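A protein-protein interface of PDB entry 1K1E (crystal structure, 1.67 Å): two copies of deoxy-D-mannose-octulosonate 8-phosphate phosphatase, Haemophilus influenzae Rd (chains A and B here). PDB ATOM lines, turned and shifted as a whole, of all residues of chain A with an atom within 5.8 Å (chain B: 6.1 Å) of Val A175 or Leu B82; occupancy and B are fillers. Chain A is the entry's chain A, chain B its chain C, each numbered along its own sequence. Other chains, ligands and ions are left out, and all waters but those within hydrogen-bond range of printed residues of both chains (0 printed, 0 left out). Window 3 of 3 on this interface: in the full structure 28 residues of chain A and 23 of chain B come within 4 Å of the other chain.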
ATOM      1  N   GLY A 170      19.836 -20.504  19.399  1.00  0.00           N
ATOM      2  CA  GLY A 170      19.297 -19.192  19.075  1.00  0.00           C
ATOM      3  C   GLY A 170      19.002 -18.368  20.313  1.00  0.00           C
ATOM      4  O   GLY A 170      19.180 -17.137  20.322  1.00  0.00           O
ATOM      5  N   PHE A 171      18.503 -19.031  21.352  1.00  0.00           N
ATOM      6  CA  PHE A 171      18.163 -18.322  22.575  1.00  0.00           C
ATOM      7  C   PHE A 171      19.412 -17.764  23.228  1.00  0.00           C
ATOM      8  O   PHE A 171      19.446 -16.598  23.679  1.00  0.00           O
ATOM      9  CB  PHE A 171      17.446 -19.258  23.557  1.00  0.00           C
ATOM     10  CG  PHE A 171      17.069 -18.587  24.844  1.00  0.00           C
ATOM     11  CD1 PHE A 171      15.959 -17.760  24.921  1.00  0.00           C
ATOM     12  CD2 PHE A 171      17.898 -18.689  25.953  1.00  0.00           C
ATOM     13  CE1 PHE A 171      15.704 -17.029  26.106  1.00  0.00           C
ATOM     14  CE2 PHE A 171      17.651 -17.983  27.116  1.00  0.00           C
ATOM     15  CZ  PHE A 171      16.563 -17.147  27.204  1.00  0.00           C
ATOM     16  N   LEU A 172      20.430 -18.625  23.320  1.00  0.00           N
ATOM     17  CA  LEU A 172      21.671 -18.229  23.944  1.00  0.00           C
ATOM     18  C   LEU A 172      22.326 -17.047  23.240  1.00  0.00           C
ATOM     19  O   LEU A 172      22.893 -16.199  23.881  1.00  0.00           O
ATOM     20  CB  LEU A 172      22.620 -19.431  24.075  1.00  0.00           C
ATOM     21  CG  LEU A 172      22.102 -20.464  25.114  1.00  0.00           C
ATOM     22  CD1 LEU A 172      22.944 -21.737  25.038  1.00  0.00           C
ATOM     23  CD2 LEU A 172      22.110 -19.866  26.558  1.00  0.00           C
ATOM     24  N   LYS A 173      22.202 -16.957  21.931  1.00  0.00           N
ATOM     25  CA  LYS A 173      22.780 -15.810  21.235  1.00  0.00           C
ATOM     26  C   LYS A 173      22.193 -14.485  21.737  1.00  0.00           C
ATOM     27  O   LYS A 173      22.875 -13.432  21.701  1.00  0.00           O
ATOM     28  CB  LYS A 173      22.500 -15.944  19.745  1.00  0.00           C
ATOM     29  CG  LYS A 173      23.123 -17.169  19.101  1.00  0.00           C
ATOM     30  CD  LYS A 173      23.197 -16.941  17.598  1.00  0.00           C
ATOM     31  CE  LYS A 173      24.362 -17.619  16.950  1.00  0.00           C
ATOM     32  NZ  LYS A 173      23.829 -18.714  16.115  1.00  0.00           N
ATOM     33  N   SER A 174      20.959 -14.544  22.262  1.00  0.00           N
ATOM     34  CA  SER A 174      20.265 -13.328  22.713  1.00  0.00           C
ATOM     35  C   SER A 174      20.025 -13.196  24.211  1.00  0.00           C
ATOM     36  O   SER A 174      19.490 -12.174  24.653  1.00  0.00           O
ATOM     37  CB  SER A 174      18.901 -13.212  22.028  1.00  0.00           C
ATOM     38  OG  SER A 174      19.005 -12.914  20.639  1.00  0.00           O
ATOM     39  N   VAL A 175      20.463 -14.181  24.992  1.00  0.00           N
ATOM     40  CA  VAL A 175      20.215 -14.206  26.439  1.00  0.00           C
ATOM     41  C   VAL A 175      20.568 -12.923  27.195  1.00  0.00           C
ATOM     42  O   VAL A 175      19.846 -12.534  28.130  1.00  0.00           O
ATOM     43  CB  VAL A 175      20.921 -15.409  27.087  1.00  0.00           C
ATOM     44  CG1 VAL A 175      22.434 -15.191  27.094  1.00  0.00           C
ATOM     45  CG2 VAL A 175      20.341 -15.645  28.495  1.00  0.00           C
ATOM     46  N   LYS A 176      21.659 -12.250  26.811  1.00  0.00           N
ATOM     47  CA  LYS A 176      22.025 -11.013  27.531  1.00  0.00           C
ATOM     48  C   LYS A 176      20.845 -10.020  27.593  1.00  0.00           C
ATOM     49  O   LYS A 176      20.771  -9.160  28.494  1.00  0.00           O
ATOM     50  CB  LYS A 176      23.249 -10.328  26.871  1.00  0.00           C
ATOM     51  N   SER A 177      19.900 -10.166  26.659  1.00  0.00           N
ATOM     52  CA  SER A 177      18.748  -9.251  26.601  1.00  0.00           C
ATOM     53  C   SER A 177      17.400  -9.815  27.031  1.00  0.00           C
ATOM     54  O   SER A 177      16.385  -9.132  26.928  1.00  0.00           O
ATOM     55  CB  SER A 177      18.653  -8.709  25.173  1.00  0.00           C
ATOM     56  OG  SER A 177      19.929  -8.210  24.806  1.00  0.00           O
ATOM     57  N   MET A 178      17.390 -11.039  27.555  1.00  0.00           N
ATOM     58  CA  MET A 178      16.139 -11.698  27.934  1.00  0.00           C
ATOM     59  C   MET A 178      15.682 -11.607  29.416  1.00  0.00           C
ATOM     60  O   MET A 178      14.792 -12.363  29.842  1.00  0.00           O
ATOM     61  CB  MET A 178      16.219 -13.176  27.518  1.00  0.00           C
ATOM     62  CG  MET A 178      16.523 -13.405  26.036  1.00  0.00           C
ATOM     63  SD  MET A 178      15.189 -12.864  24.955  1.00  0.00           S
ATOM     64  CE  MET A 178      15.972 -11.431  24.140  1.00  0.00           C
ATOM     65  N   GLY A 179      16.261 -10.688  30.196  1.00  0.00           N
ATOM     66  CA  GLY A 179      15.833 -10.591  31.589  1.00  0.00           C
ATOM     67  C   GLY A 179      14.568  -9.750  31.714  1.00  0.00           C
ATOM     68  O   GLY A 179      14.293  -8.952  30.829  1.00  0.00           O
ATOM     69  N   SER B  58      16.499 -20.910  38.675  1.00  0.00           N
ATOM     70  CA  SER B  58      15.617 -19.839  38.288  1.00  0.00           C
ATOM     71  C   SER B  58      16.465 -18.635  37.888  1.00  0.00           C
ATOM     72  O   SER B  58      17.441 -18.314  38.562  1.00  0.00           O
ATOM     73  CB  SER B  58      14.779 -19.408  39.474  1.00  0.00           C
ATOM     74  OG  SER B  58      13.931 -18.317  39.114  1.00  0.00           O
ATOM     75  N   GLY B  59      16.081 -18.000  36.803  1.00  0.00           N
ATOM     76  CA  GLY B  59      16.763 -16.766  36.429  1.00  0.00           C
ATOM     77  C   GLY B  59      16.299 -15.557  37.256  1.00  0.00           C
ATOM     78  O   GLY B  59      16.784 -14.402  37.058  1.00  0.00           O
ATOM     79  N   ARG B  60      15.351 -15.761  38.163  1.00  0.00           N
ATOM     80  CA  ARG B  60      14.835 -14.654  38.988  1.00  0.00           C
ATOM     81  C   ARG B  60      15.209 -15.101  40.423  1.00  0.00           C
ATOM     82  O   ARG B  60      15.263 -16.285  40.705  1.00  0.00           O
ATOM     83  CB  ARG B  60      13.293 -14.520  38.820  1.00  0.00           C
ATOM     84  CG  ARG B  60      12.820 -14.000  37.428  1.00  0.00           C
ATOM     85  CD  ARG B  60      11.272 -13.759  37.219  1.00  0.00           C
ATOM     86  NE  ARG B  60      10.737 -12.517  37.787  1.00  0.00           N
ATOM     87  CZ  ARG B  60      10.913 -11.276  37.294  1.00  0.00           C
ATOM     88  NH1 ARG B  60      11.624 -11.049  36.186  1.00  0.00           N
ATOM     89  NH2 ARG B  60      10.364 -10.246  37.930  1.00  0.00           N
ATOM     90  N   GLY B  80      19.063 -16.383  39.661  1.00  0.00           N
ATOM     91  CA  GLY B  80      19.654 -15.128  39.198  1.00  0.00           C
ATOM     92  C   GLY B  80      20.580 -15.256  38.029  1.00  0.00           C
ATOM     93  O   GLY B  80      21.292 -14.318  37.667  1.00  0.00           O
ATOM     94  N   LYS B  81      20.633 -16.432  37.461  1.00  0.00           N
ATOM     95  CA  LYS B  81      21.429 -16.643  36.268  1.00  0.00           C
ATOM     96  C   LYS B  81      20.464 -17.070  35.128  1.00  0.00           C
ATOM     97  O   LYS B  81      19.747 -18.122  35.209  1.00  0.00           O
ATOM     98  CB  LYS B  81      22.484 -17.699  36.547  1.00  0.00           C
ATOM     99  CG  LYS B  81      23.367 -17.981  35.378  1.00  0.00           C
ATOM    100  CD  LYS B  81      24.614 -18.684  35.810  1.00  0.00           C
ATOM    101  CE  LYS B  81      25.481 -18.968  34.583  1.00  0.00           C
ATOM    102  NZ  LYS B  81      26.886 -19.293  34.931  1.00  0.00           N
ATOM    103  N   LEU B  82      20.471 -16.281  34.055  1.00  0.00           N
ATOM    104  CA  LEU B  82      19.611 -16.499  32.854  1.00  0.00           C
ATOM    105  C   LEU B  82      20.012 -17.576  31.851  1.00  0.00           C
ATOM    106  O   LEU B  82      19.157 -18.102  31.048  1.00  0.00           O
ATOM    107  CB  LEU B  82      19.522 -15.212  32.051  1.00  0.00           C
ATOM    108  CG  LEU B  82      18.821 -14.024  32.653  1.00  0.00           C
ATOM    109  CD1 LEU B  82      18.564 -13.097  31.520  1.00  0.00           C
ATOM    110  CD2 LEU B  82      17.483 -14.415  33.330  1.00  0.00           C
ATOM    111  N   GLU B  83      21.314 -17.854  31.863  1.00  0.00           N
ATOM    112  CA  GLU B  83      21.910 -18.822  30.982  1.00  0.00           C
ATOM    113  C   GLU B  83      22.003 -20.069  31.873  1.00  0.00           C
ATOM    114  O   GLU B  83      22.843 -20.197  32.795  1.00  0.00           O
ATOM    115  CB  GLU B  83      23.258 -18.236  30.517  1.00  0.00           C
ATOM    116  CG  GLU B  83      24.000 -19.043  29.536  1.00  0.00           C
ATOM    117  CD  GLU B  83      24.871 -20.058  30.213  1.00  0.00           C
ATOM    118  OE1 GLU B  83      25.850 -19.635  30.882  1.00  0.00           O
ATOM    119  OE2 GLU B  83      24.570 -21.270  30.092  1.00  0.00           O
ATOM    120  N   LYS B  84      21.095 -20.992  31.594  1.00  0.00           N
ATOM    121  CA  LYS B  84      20.964 -22.170  32.419  1.00  0.00           C
ATOM    122  C   LYS B  84      21.848 -23.330  32.065  1.00  0.00           C
ATOM    123  O   LYS B  84      21.962 -24.246  32.863  1.00  0.00           O
ATOM    124  CB  LYS B  84      19.476 -22.557  32.404  1.00  0.00           C
ATOM    125  CG  LYS B  84      18.593 -21.533  33.090  1.00  0.00           C
ATOM    126  CD  LYS B  84      17.128 -22.010  33.077  1.00  0.00           C
ATOM    127  CE  LYS B  84      16.194 -21.068  33.840  1.00  0.00           C
ATOM    128  NZ  LYS B  84      14.884 -21.717  34.196  1.00  0.00           N
ATOM    129  N   VAL B 110      13.904 -20.391  27.699  1.00  0.00           N
ATOM    130  CA  VAL B 110      15.032 -20.275  28.572  1.00  0.00           C
ATOM    131  C   VAL B 110      15.503 -21.629  29.002  1.00  0.00           C
ATOM    132  O   VAL B 110      16.704 -21.783  29.313  1.00  0.00           O
ATOM    133  CB  VAL B 110      14.714 -19.520  29.870  1.00  0.00           C
ATOM    134  CG1 VAL B 110      16.025 -19.110  30.612  1.00  0.00           C
ATOM    135  CG2 VAL B 110      13.820 -18.321  29.586  1.00  0.00           C
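Among the printed residues, pairs that only touch across the chains: Phe A171 with Val B110 (3.7 Å), Leu A172 with Glu B83 (3.6 Å), Val A175 with Leu B82 (3.7 Å), Met A178 with Leu B82 (3.9 Å) and Gly A179 with Leu B82 (3.6 Å).
Of the 9 printed residues of chain B, 3 touch a printed residue of chain A. Hydrophobic or aromatic side chains of chain B within 4 Å of the printed part of chain A: Leu B82 and Val B110. Among the printed residues, 5 pairs touch across the chains.
No position is printed for both chains.
Of chain B, only Leu B82 comes within 4 Å of Val A175. Of the printed residues of chain A, Val B110 touches Phe A171 (3.7 Å). Printed residues of chain B within 4 Å of Leu A172: Glu B83 (3.6 Å). Of the printed residues of chain B, Phe A171 touches Val B110 (3.7 Å). The nearest printed residue of chain B that does not touch Leu A172 is Lys B84 (5.3 Å).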
